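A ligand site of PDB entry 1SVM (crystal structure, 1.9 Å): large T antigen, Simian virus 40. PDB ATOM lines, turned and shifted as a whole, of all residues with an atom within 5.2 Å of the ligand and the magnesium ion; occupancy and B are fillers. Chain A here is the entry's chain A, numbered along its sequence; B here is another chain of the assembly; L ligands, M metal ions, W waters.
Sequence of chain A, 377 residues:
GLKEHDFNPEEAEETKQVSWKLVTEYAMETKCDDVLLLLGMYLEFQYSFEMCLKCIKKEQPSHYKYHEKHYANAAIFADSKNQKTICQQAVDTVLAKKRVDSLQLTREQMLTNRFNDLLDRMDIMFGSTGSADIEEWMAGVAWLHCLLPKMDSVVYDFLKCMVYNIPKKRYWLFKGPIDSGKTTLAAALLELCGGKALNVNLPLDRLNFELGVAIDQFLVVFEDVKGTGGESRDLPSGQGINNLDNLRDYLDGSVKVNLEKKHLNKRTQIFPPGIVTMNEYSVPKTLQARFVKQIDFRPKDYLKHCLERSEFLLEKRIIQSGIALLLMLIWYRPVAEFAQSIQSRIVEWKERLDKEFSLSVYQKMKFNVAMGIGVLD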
ATOM      1  N   TRP A 143      20.199 -31.233 -12.262  1.00  0.00           N
ATOM      2  CA  TRP A 143      20.782 -29.896 -12.268  1.00  0.00           C
ATOM      3  C   TRP A 143      19.807 -28.870 -11.696  1.00  0.00           C
ATOM      4  O   TRP A 143      20.182 -28.027 -10.883  1.00  0.00           O
ATOM      5  CB  TRP A 143      21.165 -29.494 -13.703  1.00  0.00           C
ATOM      6  CG  TRP A 143      21.947 -28.201 -13.799  1.00  0.00           C
ATOM      7  CD1 TRP A 143      23.308 -28.059 -13.812  1.00  0.00           C
ATOM      8  CD2 TRP A 143      21.407 -26.870 -13.877  1.00  0.00           C
ATOM      9  NE1 TRP A 143      23.651 -26.724 -13.903  1.00  0.00           N
ATOM     10  CE2 TRP A 143      22.500 -25.979 -13.936  1.00  0.00           C
ATOM     11  CE3 TRP A 143      20.107 -26.351 -13.895  1.00  0.00           C
ATOM     12  CZ2 TRP A 143      22.337 -24.584 -14.025  1.00  0.00           C
ATOM     13  CZ3 TRP A 143      19.934 -24.969 -13.979  1.00  0.00           C
ATOM     14  CH2 TRP A 143      21.043 -24.102 -14.048  1.00  0.00           C
ATOM     15  N   LEU A 147      19.519 -25.956  -8.354  1.00  0.00           N
ATOM     16  CA  LEU A 147      19.442 -24.522  -8.607  1.00  0.00           C
ATOM     17  C   LEU A 147      18.848 -23.726  -7.437  1.00  0.00           C
ATOM     18  O   LEU A 147      19.284 -22.605  -7.160  1.00  0.00           O
ATOM     19  CB  LEU A 147      18.601 -24.268  -9.864  1.00  0.00           C
ATOM     20  CG  LEU A 147      18.361 -22.805 -10.225  1.00  0.00           C
ATOM     21  CD1 LEU A 147      19.694 -22.121 -10.531  1.00  0.00           C
ATOM     22  CD2 LEU A 147      17.429 -22.725 -11.440  1.00  0.00           C
ATOM     23  N   GLY A 176      17.601 -11.448  -9.002  1.00  0.00           N
ATOM     24  CA  GLY A 176      18.983 -11.865  -8.890  1.00  0.00           C
ATOM     25  C   GLY A 176      19.873 -11.308  -9.982  1.00  0.00           C
ATOM     26  O   GLY A 176      19.385 -10.726 -10.951  1.00  0.00           O
ATOM     27  N   PRO A 177      21.190 -11.507  -9.850  1.00  0.00           N
ATOM     28  CA  PRO A 177      22.210 -11.048 -10.801  1.00  0.00           C
ATOM     29  C   PRO A 177      22.135 -11.787 -12.133  1.00  0.00           C
ATOM     30  O   PRO A 177      21.399 -12.764 -12.265  1.00  0.00           O
ATOM     31  CB  PRO A 177      23.530 -11.358 -10.084  1.00  0.00           C
ATOM     32  CG  PRO A 177      23.141 -11.458  -8.635  1.00  0.00           C
ATOM     33  CD  PRO A 177      21.828 -12.150  -8.692  1.00  0.00           C
ATOM     34  N   ILE A 178      22.923 -11.316 -13.087  1.00  0.00           N
ATOM     35  CA  ILE A 178      22.996 -11.924 -14.406  1.00  0.00           C
ATOM     36  C   ILE A 178      23.367 -13.395 -14.258  1.00  0.00           C
ATOM     37  O   ILE A 178      24.159 -13.759 -13.384  1.00  0.00           O
ATOM     38  CB  ILE A 178      24.064 -11.212 -15.276  1.00  0.00           C
ATOM     39  CG1 ILE A 178      23.616  -9.762 -15.552  1.00  0.00           C
ATOM     40  CG2 ILE A 178      24.282 -11.962 -16.583  1.00  0.00           C
ATOM     41  CD1 ILE A 178      24.656  -8.926 -16.274  1.00  0.00           C
ATOM     42  N   ASP A 179      22.784 -14.236 -15.106  1.00  0.00           N
ATOM     43  CA  ASP A 179      23.023 -15.688 -15.106  1.00  0.00           C
ATOM     44  C   ASP A 179      22.903 -16.391 -13.760  1.00  0.00           C
ATOM     45  O   ASP A 179      23.792 -17.150 -13.356  1.00  0.00           O
ATOM     46  CB  ASP A 179      24.386 -16.003 -15.729  1.00  0.00           C
ATOM     47  CG  ASP A 179      24.496 -15.579 -17.185  1.00  0.00           C
ATOM     48  OD1 ASP A 179      23.435 -15.426 -17.850  1.00  0.00           O
ATOM     49  OD2 ASP A 179      25.630 -15.394 -17.676  1.00  0.00           O
ATOM     50  N   SER A 180      21.790 -16.168 -13.073  1.00  0.00           N
ATOM     51  CA  SER A 180      21.541 -16.800 -11.789  1.00  0.00           C
ATOM     52  C   SER A 180      20.442 -17.856 -11.924  1.00  0.00           C
ATOM     53  O   SER A 180      20.138 -18.571 -10.973  1.00  0.00           O
ATOM     54  CB  SER A 180      21.188 -15.758 -10.728  1.00  0.00           C
ATOM     55  OG  SER A 180      20.178 -14.866 -11.178  1.00  0.00           O
ATOM     56  N   GLY A 181      19.836 -17.957 -13.115  1.00  0.00           N
ATOM     57  CA  GLY A 181      18.806 -18.954 -13.345  1.00  0.00           C
ATOM     58  C   GLY A 181      17.353 -18.500 -13.405  1.00  0.00           C
ATOM     59  O   GLY A 181      16.444 -19.326 -13.495  1.00  0.00           O
ATOM     60  N   LYS A 182      17.127 -17.195 -13.373  1.00  0.00           N
ATOM     61  CA  LYS A 182      15.765 -16.651 -13.389  1.00  0.00           C
ATOM     62  C   LYS A 182      14.979 -17.070 -14.634  1.00  0.00           C
ATOM     63  O   LYS A 182      13.901 -17.648 -14.538  1.00  0.00           O
ATOM     64  CB  LYS A 182      15.812 -15.118 -13.309  1.00  0.00           C
ATOM     65  CG  LYS A 182      16.510 -14.584 -12.056  1.00  0.00           C
ATOM     66  CD  LYS A 182      16.427 -13.064 -11.969  1.00  0.00           C
ATOM     67  CE  LYS A 182      17.128 -12.383 -13.134  1.00  0.00           C
ATOM     68  NZ  LYS A 182      18.558 -12.766 -13.229  1.00  0.00           N
ATOM     69  N   THR A 183      15.541 -16.767 -15.800  1.00  0.00           N
ATOM     70  CA  THR A 183      14.914 -17.089 -17.077  1.00  0.00           C
ATOM     71  C   THR A 183      14.824 -18.598 -17.296  1.00  0.00           C
ATOM     72  O   THR A 183      13.831 -19.101 -17.803  1.00  0.00           O
ATOM     73  CB  THR A 183      15.701 -16.452 -18.232  1.00  0.00           C
ATOM     74  OG1 THR A 183      15.564 -15.037 -18.159  1.00  0.00           O
ATOM     75  CG2 THR A 183      15.195 -16.956 -19.590  1.00  0.00           C
ATOM     76  N   THR A 184      15.865 -19.320 -16.894  1.00  0.00           N
ATOM     77  CA  THR A 184      15.861 -20.762 -17.058  1.00  0.00           C
ATOM     78  C   THR A 184      14.640 -21.369 -16.384  1.00  0.00           C
ATOM     79  O   THR A 184      13.892 -22.124 -16.991  1.00  0.00           O
ATOM     80  CB  THR A 184      17.160 -21.389 -16.489  1.00  0.00           C
ATOM     81  OG1 THR A 184      18.297 -20.819 -17.146  1.00  0.00           O
ATOM     82  CG2 THR A 184      17.165 -22.908 -16.708  1.00  0.00           C
ATOM     83  N   GLU A 223       9.234 -10.915 -18.414  1.00  0.00           N
ATOM     84  CA  GLU A 223      10.677 -11.161 -18.451  1.00  0.00           C
ATOM     85  C   GLU A 223      11.577  -9.934 -18.408  1.00  0.00           C
ATOM     86  O   GLU A 223      11.331  -8.924 -19.075  1.00  0.00           O
ATOM     87  CB  GLU A 223      11.028 -11.973 -19.707  1.00  0.00           C
ATOM     88  CG  GLU A 223      11.350 -13.430 -19.436  1.00  0.00           C
ATOM     89  CD  GLU A 223      12.666 -13.604 -18.696  1.00  0.00           C
ATOM     90  OE1 GLU A 223      13.728 -13.497 -19.332  1.00  0.00           O
ATOM     91  OE2 GLU A 223      12.625 -13.852 -17.471  1.00  0.00           O
ATOM     92  N   ASP A 224      12.619 -10.049 -17.604  1.00  0.00           N
ATOM     93  CA  ASP A 224      13.636  -9.015 -17.467  1.00  0.00           C
ATOM     94  C   ASP A 224      13.136  -7.573 -17.365  1.00  0.00           C
ATOM     95  O   ASP A 224      13.565  -6.706 -18.124  1.00  0.00           O
ATOM     96  CB  ASP A 224      14.598  -9.156 -18.644  1.00  0.00           C
ATOM     97  CG  ASP A 224      16.036  -9.209 -18.204  1.00  0.00           C
ATOM     98  OD1 ASP A 224      16.855  -9.809 -18.927  1.00  0.00           O
ATOM     99  OD2 ASP A 224      16.340  -8.651 -17.134  1.00  0.00           O
ATOM    100  N   THR A 277      10.512 -11.413 -13.600  1.00  0.00           N
ATOM    101  CA  THR A 277      11.931 -11.664 -13.379  1.00  0.00           C
ATOM    102  C   THR A 277      12.653 -10.332 -13.575  1.00  0.00           C
ATOM    103  O   THR A 277      12.286  -9.546 -14.453  1.00  0.00           O
ATOM    104  CB  THR A 277      12.529 -12.697 -14.366  1.00  0.00           C
ATOM    105  OG1 THR A 277      12.717 -12.104 -15.652  1.00  0.00           O
ATOM    106  CG2 THR A 277      11.627 -13.912 -14.472  1.00  0.00           C
ATOM    107  N   ASN A 279      16.621  -7.952 -12.512  1.00  0.00           N
ATOM    108  CA  ASN A 279      17.916  -7.886 -11.871  1.00  0.00           C
ATOM    109  C   ASN A 279      17.660  -7.152 -10.544  1.00  0.00           C
ATOM    110  O   ASN A 279      16.512  -6.849 -10.219  1.00  0.00           O
ATOM    111  CB  ASN A 279      18.926  -7.142 -12.750  1.00  0.00           C
ATOM    112  CG  ASN A 279      19.404  -7.991 -13.906  1.00  0.00           C
ATOM    113  OD1 ASN A 279      19.327  -7.597 -15.070  1.00  0.00           O
ATOM    114  ND2 ASN A 279      19.904  -9.187 -13.591  1.00  0.00           N
ATOM    115  N   ARG A 298      20.914 -17.077  -7.070  1.00  0.00           N
ATOM    116  CA  ARG A 298      22.326 -16.839  -6.830  1.00  0.00           C
ATOM    117  C   ARG A 298      23.205 -17.681  -7.755  1.00  0.00           C
ATOM    118  O   ARG A 298      23.010 -18.889  -7.890  1.00  0.00           O
ATOM    119  CB  ARG A 298      22.650 -17.167  -5.372  1.00  0.00           C
ATOM    120  CG  ARG A 298      21.702 -16.511  -4.379  1.00  0.00           C
ATOM    121  CD  ARG A 298      21.882 -17.027  -2.951  1.00  0.00           C
ATOM    122  NE  ARG A 298      23.122 -16.554  -2.334  1.00  0.00           N
ATOM    123  CZ  ARG A 298      23.455 -16.783  -1.072  1.00  0.00           C
ATOM    124  NH1 ARG A 298      22.648 -17.478  -0.275  1.00  0.00           N
ATOM    125  NH2 ARG A 298      24.611 -16.314  -0.591  1.00  0.00           N
ATOM    126  N   PRO A 299      24.165 -17.043  -8.422  1.00  0.00           N
ATOM    127  CA  PRO A 299      25.052 -17.780  -9.321  1.00  0.00           C
ATOM    128  C   PRO A 299      25.858 -18.777  -8.486  1.00  0.00           C
ATOM    129  O   PRO A 299      26.278 -18.457  -7.379  1.00  0.00           O
ATOM    130  CB  PRO A 299      25.942 -16.696  -9.913  1.00  0.00           C
ATOM    131  CG  PRO A 299      25.097 -15.466  -9.821  1.00  0.00           C
ATOM    132  CD  PRO A 299      24.464 -15.603  -8.470  1.00  0.00           C
ATOM    133  N   LYS A 300      26.034 -19.982  -9.005  1.00  0.00           N
ATOM    134  CA  LYS A 300      26.797 -21.013  -8.302  1.00  0.00           C
ATOM    135  C   LYS A 300      27.849 -21.553  -9.255  1.00  0.00           C
ATOM    136  O   LYS A 300      27.529 -22.124 -10.296  1.00  0.00           O
ATOM    137  CB  LYS A 300      25.868 -22.139  -7.838  1.00  0.00           C
ATOM    138  CG  LYS A 300      24.793 -21.676  -6.872  1.00  0.00           C
ATOM    139  CD  LYS A 300      23.868 -22.827  -6.474  1.00  0.00           C
ATOM    140  CE  LYS A 300      22.811 -22.368  -5.487  1.00  0.00           C
ATOM    141  NZ  LYS A 300      21.913 -23.489  -5.078  1.00  0.00           N
ATOM    142  N   ASP A 301      29.122 -21.363  -8.893  1.00  0.00           N
ATOM    143  CA  ASP A 301      30.228 -21.819  -9.722  1.00  0.00           C
ATOM    144  C   ASP A 301      30.120 -23.266 -10.179  1.00  0.00           C
ATOM    145  O   ASP A 301      30.422 -23.581 -11.328  1.00  0.00           O
ATOM    146  CB  ASP A 301      31.552 -21.591  -8.995  1.00  0.00           C
ATOM    147  CG  ASP A 301      31.940 -20.124  -8.934  1.00  0.00           C
ATOM    148  OD1 ASP A 301      32.022 -19.484 -10.001  1.00  0.00           O
ATOM    149  OD2 ASP A 301      32.163 -19.619  -7.813  1.00  0.00           O
ATOM    150  N   LEU A 303      27.423 -25.018 -10.655  1.00  0.00           N
ATOM    151  CA  LEU A 303      26.343 -25.201 -11.627  1.00  0.00           C
ATOM    152  C   LEU A 303      26.892 -24.845 -13.008  1.00  0.00           C
ATOM    153  O   LEU A 303      26.593 -25.503 -14.000  1.00  0.00           O
ATOM    154  CB  LEU A 303      25.149 -24.285 -11.296  1.00  0.00           C
ATOM    155  CG  LEU A 303      24.345 -24.631 -10.033  1.00  0.00           C
ATOM    156  CD1 LEU A 303      23.216 -23.616  -9.852  1.00  0.00           C
ATOM    157  CD2 LEU A 303      23.773 -26.041 -10.139  1.00  0.00           C
ATOM    158  N   LYS A 304      27.716 -23.816 -13.038  1.00  0.00           N
ATOM    159  CA  LYS A 304      28.337 -23.361 -14.278  1.00  0.00           C
ATOM    160  C   LYS A 304      29.382 -24.370 -14.746  1.00  0.00           C
ATOM    161  O   LYS A 304      29.424 -24.723 -15.923  1.00  0.00           O
ATOM    162  CB  LYS A 304      28.980 -21.993 -14.043  1.00  0.00           C
ATOM    163  CG  LYS A 304      29.716 -21.431 -15.246  1.00  0.00           C
ATOM    164  CD  LYS A 304      30.184 -20.014 -14.971  1.00  0.00           C
ATOM    165  CE  LYS A 304      31.061 -19.942 -13.731  1.00  0.00           C
ATOM    166  NZ  LYS A 304      31.368 -18.533 -13.334  1.00  0.00           N
ATOM    167  N   LEU A 307      27.659 -27.505 -16.257  1.00  0.00           N
ATOM    168  CA  LEU A 307      27.111 -27.304 -17.603  1.00  0.00           C
ATOM    169  C   LEU A 307      28.195 -27.345 -18.673  1.00  0.00           C
ATOM    170  O   LEU A 307      27.971 -27.880 -19.762  1.00  0.00           O
ATOM    171  CB  LEU A 307      26.359 -25.972 -17.675  1.00  0.00           C
ATOM    172  CG  LEU A 307      25.022 -25.886 -16.934  1.00  0.00           C
ATOM    173  CD1 LEU A 307      24.446 -24.499 -17.102  1.00  0.00           C
ATOM    174  CD2 LEU A 307      24.062 -26.933 -17.468  1.00  0.00           C
ATOM    175  N   LEU A 314      22.127 -27.673 -22.370  1.00  0.00           N
ATOM    176  CA  LEU A 314      21.836 -26.387 -22.974  1.00  0.00           C
ATOM    177  C   LEU A 314      21.566 -26.534 -24.461  1.00  0.00           C
ATOM    178  O   LEU A 314      20.668 -25.880 -24.995  1.00  0.00           O
ATOM    179  CB  LEU A 314      23.003 -25.413 -22.754  1.00  0.00           C
ATOM    180  CG  LEU A 314      23.214 -24.898 -21.334  1.00  0.00           C
ATOM    181  CD1 LEU A 314      24.401 -23.952 -21.282  1.00  0.00           C
ATOM    182  CD2 LEU A 314      21.954 -24.182 -20.856  1.00  0.00           C
ATOM    183  N   ILE A 319      17.299 -28.077 -19.394  1.00  0.00           N
ATOM    184  CA  ILE A 319      17.073 -27.412 -18.100  1.00  0.00           C
ATOM    185  C   ILE A 319      16.066 -26.281 -18.144  1.00  0.00           C
ATOM    186  O   ILE A 319      15.633 -25.799 -17.100  1.00  0.00           O
ATOM    187  CB  ILE A 319      18.390 -26.880 -17.479  1.00  0.00           C
ATOM    188  CG1 ILE A 319      19.129 -25.980 -18.467  1.00  0.00           C
ATOM    189  CG2 ILE A 319      19.258 -28.062 -17.045  1.00  0.00           C
ATOM    190  CD1 ILE A 319      20.333 -25.269 -17.860  1.00  0.00           C
ATOM    191  N   GLN A 320      15.678 -25.852 -19.341  1.00  0.00           N
ATOM    192  CA  GLN A 320      14.706 -24.771 -19.475  1.00  0.00           C
ATOM    193  C   GLN A 320      13.334 -25.336 -19.883  1.00  0.00           C
ATOM    194  O   GLN A 320      12.405 -24.580 -20.137  1.00  0.00           O
ATOM    195  CB  GLN A 320      15.189 -23.765 -20.519  1.00  0.00           C
ATOM    196  CG  GLN A 320      16.573 -23.195 -20.218  1.00  0.00           C
ATOM    197  CD  GLN A 320      17.714 -23.839 -21.015  1.00  0.00           C
ATOM    198  OE1 GLN A 320      17.831 -25.085 -21.100  1.00  0.00           O
ATOM    199  NE2 GLN A 320      18.565 -22.995 -21.588  1.00  0.00           N
ATOM    200  N   PRO B 167      20.468 -21.297 -25.949  1.00  0.00           N
ATOM    201  CA  PRO B 167      19.966 -20.191 -25.135  1.00  0.00           C
ATOM    202  C   PRO B 167      21.077 -19.286 -24.594  1.00  0.00           C
ATOM    203  O   PRO B 167      22.035 -19.757 -23.958  1.00  0.00           O
ATOM    204  CB  PRO B 167      19.204 -20.901 -24.018  1.00  0.00           C
ATOM    205  CG  PRO B 167      18.620 -22.075 -24.720  1.00  0.00           C
ATOM    206  CD  PRO B 167      19.804 -22.565 -25.578  1.00  0.00           C
ATOM    207  N   LYS B 168      20.940 -17.999 -24.865  1.00  0.00           N
ATOM    208  CA  LYS B 168      21.875 -16.985 -24.413  1.00  0.00           C
ATOM    209  C   LYS B 168      23.300 -17.122 -24.946  1.00  0.00           C
ATOM    210  O   LYS B 168      24.221 -16.500 -24.415  1.00  0.00           O
ATOM    211  CB  LYS B 168      21.888 -16.932 -22.883  1.00  0.00           C
ATOM    212  CG  LYS B 168      22.112 -15.533 -22.338  1.00  0.00           C
ATOM    213  CD  LYS B 168      21.762 -15.475 -20.879  1.00  0.00           C
ATOM    214  CE  LYS B 168      21.736 -14.043 -20.374  1.00  0.00           C
ATOM    215  NZ  LYS B 168      21.301 -13.989 -18.964  1.00  0.00           N
ATOM    216  N   LYS B 169      23.474 -17.925 -25.996  1.00  0.00           N
ATOM    217  CA  LYS B 169      24.778 -18.120 -26.626  1.00  0.00           C
ATOM    218  C   LYS B 169      24.539 -18.150 -28.124  1.00  0.00           C
ATOM    219  O   LYS B 169      25.106 -18.987 -28.840  1.00  0.00           O
ATOM    220  CB  LYS B 169      25.401 -19.455 -26.173  1.00  0.00           C
ATOM    221  CG  LYS B 169      25.688 -19.555 -24.679  1.00  0.00           C
ATOM    222  CD  LYS B 169      26.399 -20.868 -24.356  1.00  0.00           C
ATOM    223  CE  LYS B 169      26.665 -21.015 -22.865  1.00  0.00           C
ATOM    224  NZ  LYS B 169      27.503 -19.889 -22.340  1.00  0.00           N
ATOM    225  N   ASP B 252      18.198 -13.617 -25.905  1.00  0.00           N
ATOM    226  CA  ASP B 252      18.374 -14.865 -25.134  1.00  0.00           C
ATOM    227  C   ASP B 252      17.860 -16.092 -25.872  1.00  0.00           C
ATOM    228  O   ASP B 252      18.508 -17.142 -25.875  1.00  0.00           O
ATOM    229  CB  ASP B 252      17.638 -14.789 -23.789  1.00  0.00           C
ATOM    230  CG  ASP B 252      18.356 -13.949 -22.762  1.00  0.00           C
ATOM    231  OD1 ASP B 252      19.465 -13.470 -23.051  1.00  0.00           O
ATOM    232  OD2 ASP B 252      17.803 -13.760 -21.649  1.00  0.00           O
ATOM    233  N   SER B 254      15.327 -17.932 -25.021  1.00  0.00           N
ATOM    234  CA  SER B 254      14.880 -18.953 -24.070  1.00  0.00           C
ATOM    235  C   SER B 254      13.364 -19.067 -24.067  1.00  0.00           C
ATOM    236  O   SER B 254      12.816 -20.179 -24.080  1.00  0.00           O
ATOM    237  CB  SER B 254      15.371 -18.624 -22.661  1.00  0.00           C
ATOM    238  OG  SER B 254      16.779 -18.771 -22.570  1.00  0.00           O
ATOM    239  N   ALA B 289      26.330  -9.784 -22.055  1.00  0.00           N
ATOM    240  CA  ALA B 289      26.048 -11.152 -21.623  1.00  0.00           C
ATOM    241  C   ALA B 289      25.276 -11.991 -22.649  1.00  0.00           C
ATOM    242  O   ALA B 289      25.208 -13.218 -22.508  1.00  0.00           O
ATOM    243  CB  ALA B 289      25.299 -11.124 -20.287  1.00  0.00           C
ATOM    244  N   ARG B 290      24.694 -11.346 -23.656  1.00  0.00           N
ATOM    245  CA  ARG B 290      23.940 -12.071 -24.691  1.00  0.00           C
ATOM    246  C   ARG B 290      24.849 -12.376 -25.877  1.00  0.00           C
ATOM    247  O   ARG B 290      24.462 -13.088 -26.794  1.00  0.00           O
ATOM    248  CB  ARG B 290      22.753 -11.244 -25.209  1.00  0.00           C
ATOM    249  CG  ARG B 290      22.047 -10.397 -24.168  1.00  0.00           C
ATOM    250  CD  ARG B 290      21.263 -11.217 -23.180  1.00  0.00           C
ATOM    251  NE  ARG B 290      21.272 -10.535 -21.898  1.00  0.00           N
ATOM    252  CZ  ARG B 290      20.435 -10.764 -20.895  1.00  0.00           C
ATOM    253  NH1 ARG B 290      19.468 -11.658 -20.995  1.00  0.00           N
ATOM    254  NH2 ARG B 290      20.576 -10.080 -19.767  1.00  0.00           N
HETATM  255  P1  LIG L   1      19.814 -12.419 -16.785  1.00  0.00           P
HETATM  256  O1  LIG L   1      18.545 -12.581 -17.565  1.00  0.00           O
HETATM  257  O2  LIG L   1      21.002 -11.923 -17.646  1.00  0.00           O
HETATM  258  O3  LIG L   1      19.533 -11.394 -15.658  1.00  0.00           O
HETATM  259  P2  LIG L   1      19.137 -14.861 -15.384  1.00  0.00           P
HETATM  260  O4  LIG L   1      19.770 -15.830 -14.504  1.00  0.00           O
HETATM  261  O5  LIG L   1      17.845 -15.106 -16.162  1.00  0.00           O
HETATM  262  O6  LIG L   1      20.163 -13.768 -15.931  1.00  0.00           O
HETATM  263  P3  LIG L   1      19.240 -16.979 -17.448  1.00  0.00           P
HETATM  264  O7  LIG L   1      19.679 -16.776 -18.842  1.00  0.00           O
HETATM  265  O8  LIG L   1      18.624 -18.227 -16.847  1.00  0.00           O
HETATM  266  O9  LIG L   1      19.864 -15.991 -16.335  1.00  0.00           O
HETATM  267  O10 LIG L   1      20.664 -17.728 -17.323  1.00  0.00           O
HETATM  268  C1  LIG L   1      20.842 -19.000 -17.935  1.00  0.00           C
HETATM  269  C2  LIG L   1      22.290 -19.367 -18.205  1.00  0.00           C
HETATM  270  O11 LIG L   1      23.152 -18.971 -17.157  1.00  0.00           O
HETATM  271  C3  LIG L   1      22.373 -20.855 -18.342  1.00  0.00           C
HETATM  272  O12 LIG L   1      22.330 -21.165 -19.722  1.00  0.00           O
HETATM  273  C4  LIG L   1      23.662 -21.240 -17.605  1.00  0.00           C
HETATM  274  O13 LIG L   1      24.810 -21.434 -18.376  1.00  0.00           O
HETATM  275  C5  LIG L   1      23.828 -20.121 -16.594  1.00  0.00           C
HETATM  276  N1  LIG L   1      23.242 -20.211 -15.198  1.00  0.00           N
HETATM  277  C6  LIG L   1      21.892 -20.217 -14.878  1.00  0.00           C
HETATM  278  N2  LIG L   1      21.793 -20.294 -13.574  1.00  0.00           N
HETATM  279  C7  LIG L   1      23.013 -20.362 -12.983  1.00  0.00           C
HETATM  280  C8  LIG L   1      23.517 -20.453 -11.670  1.00  0.00           C
HETATM  281  N3  LIG L   1      22.798 -20.450 -10.566  1.00  0.00           N
HETATM  282  N4  LIG L   1      24.897 -20.501 -11.474  1.00  0.00           N
HETATM  283  C9  LIG L   1      25.784 -20.457 -12.534  1.00  0.00           C
HETATM  284  N5  LIG L   1      25.311 -20.366 -13.827  1.00  0.00           N
HETATM  285  C10 LIG L   1      23.946 -20.320 -14.036  1.00  0.00           C
HETATM  286 MG    MG M   1      16.979 -13.711 -17.831  1.00  0.00          MG
HETATM  287  O   HOH W   1      26.666 -17.259 -13.403  1.00  0.00           O
HETATM  288  O   HOH W   2      19.999  -8.957 -17.487  1.00  0.00           O
HETATM  289  O   HOH W   3      23.546 -20.199 -21.880  1.00  0.00           O
HETATM  290  O   HOH W   4      15.649 -12.796 -16.501  1.00  0.00           O
HETATM  291  O   HOH W   5      16.871 -10.164 -15.282  1.00  0.00           O
HETATM  292  O   HOH W   6      18.420 -14.625 -19.278  1.00  0.00           O
HETATM  293  O   HOH W   7      16.222 -12.445 -19.482  1.00  0.00           O
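N of Thr 183 lies close to O5 of the ligand (2.9 Å). An oxygen (O2) of the ligand lies within salt-bridge range of the side-chain amino group (NZ) of Lys 168 of chain B. O4 of the ligand sits at hydrogen-bond distance from N of Ser 180, at 2.5 Å. A nitrogen (N3) of the ligand is in hydrogen-bond range of the backbone carbonyl oxygen (O) of Ser 180 (3.3 Å). OG of Ser 180 lies close to O4 of the ligand (3.5 Å). The backbone NH of Gly 181 is in hydrogen-bond range of an oxygen (O4) of the ligand (2.5 Å). An oxygen (O8) of the ligand is in hydrogen-bond range of the backbone NH (N) of Thr 184, 3.0 Å away. OG1 of Thr 184 sits at hydrogen-bond distance from O8 of the ligand (2.6 Å). The backbone NH (N) of Lys 300 sits at hydrogen-bond distance from a nitrogen (N4) of the ligand. The backbone NH of Asp 179 lies within hydrogen-bond range of an oxygen (O6) of the ligand, at 2.8 Å. The guanidinium group of Arg 290 of chain B is in salt-bridge range of an oxygen (O2) of the ligand, at 2.8 Å. N of Lys 182 is in hydrogen-bond range of O4 of the ligand, at 3.2 Å. O3 of the ligand is in salt-bridge range of NZ of Lys 182. An oxygen (O3) of the ligand lies within hydrogen-bond range of the side-chain amide nitrogen (ND2) of Asn 279, 3.0 Å away. A nitrogen (N3) of the ligand is in hydrogen-bond range of the backbone carbonyl oxygen (O) of Arg 298.
The side-chain carboxylate (OE1) of Glu 223 lies close to the side-chain hydroxyl (OG1) of Thr 183 (2.7 Å). OD1 of Asp 179 lies within salt-bridge range of NZ of Lys 168 of chain B, at 2.8 Å. The side-chain amino group (NZ) of Lys 182 sits at hydrogen-bond distance from the side-chain hydroxyl (OG) of Ser 180 (3.4 Å). The backbone carbonyl oxygen (O) of Pro 177 is in hydrogen-bond range of the side-chain amino group (NZ) of Lys 182 (3.0 Å). The side-chain amide nitrogen (ND2) of Asn 279 is in hydrogen-bond range of the backbone carbonyl oxygen (O) of Gly 176, 3.1 Å away. The backbone carbonyl oxygen of Leu 303 lies within hydrogen-bond range of the indole nitrogen of Trp 143. The backbone NH (N) of Asp 224 sits at hydrogen-bond distance from the side-chain hydroxyl (OG1) of Thr 277 (2.8 Å). The side-chain hydroxyl of Thr 277 sits at hydrogen-bond distance from the side-chain carboxylate of Glu 223 (2.5 Å).
Residues that only touch the ligand: Trp 143 (3.9 Å), Leu 147 (3.5 Å), Pro 177 (3.997 Å), Ile 178 (3.4 Å), Asp 224 (3.5 Å), Pro 299 (3.5 Å), Leu 303 (3.3 Å), Lys 304 (3.9 Å), Leu 307 (3.3 Å) and Leu 314 (3.2 Å). Hydrophobic or aromatic side chains within 4 Å of the ligand: Trp 143, Leu 147, Ile 178, Leu 303, Leu 307 and Leu 314. 21 residues have an atom within 4 Å of the ligand: Trp 143, Leu 147, Pro 177, Ile 178, Asp 179, Ser 180, Gly 181, Lys 182, Thr 183, Thr 184, Asp 224, Asn 279, Arg 298, Pro 299, Lys 300, Leu 303, Lys 304, Leu 307, Leu 314, Lys 168 of chain B and Arg 290 of chain B.
Residues that only touch the magnesium ion: Glu 223 (3.6 Å) and Asp 252 of chain B (3.9 Å).
The magnesium ion is bound by O1 of the ligand (1.9 Å). OG1 of Thr 183 is bound to the magnesium ion (2.0 Å). Water W4 binds the magnesium ion, 2.1 Å away. Water W7 binds the magnesium ion (2.2 Å). The magnesium ion is bound by water W6, at 2.2 Å. O5 of the ligand binds the magnesium ion.
Water W6 lies within hydrogen-bond range of an oxygen (O7) of the ligand (2.5 Å), the side-chain carboxylate of Asp 252 of chain B (2.6 Å) and the side-chain amino group of Lys 168 of chain B (3.0 Å). Water W4 lies within hydrogen-bond range of the side-chain hydroxyl (OG1) of Thr 277 (3.1 Å) and the side-chain carboxylate (OE2) of Glu 223 (3.3 Å). Water W3 lies within hydrogen-bond range of O of Pro 167 of chain B (2.6 Å) and O12 of the ligand (2.7 Å). Water W5 lies within hydrogen-bond range of OD2 of Asp 224 and O3 of the ligand. Water W2 lies within hydrogen-bond range of NH2 of Arg 290 of chain B (2.6 Å), OD1 of Asn 279 (2.9 Å) and O3 of the ligand (3.1 Å). Water W1 lies within hydrogen-bond range of O of Asp 179 (2.9 Å) and N5 of the ligand (3.4 Å).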
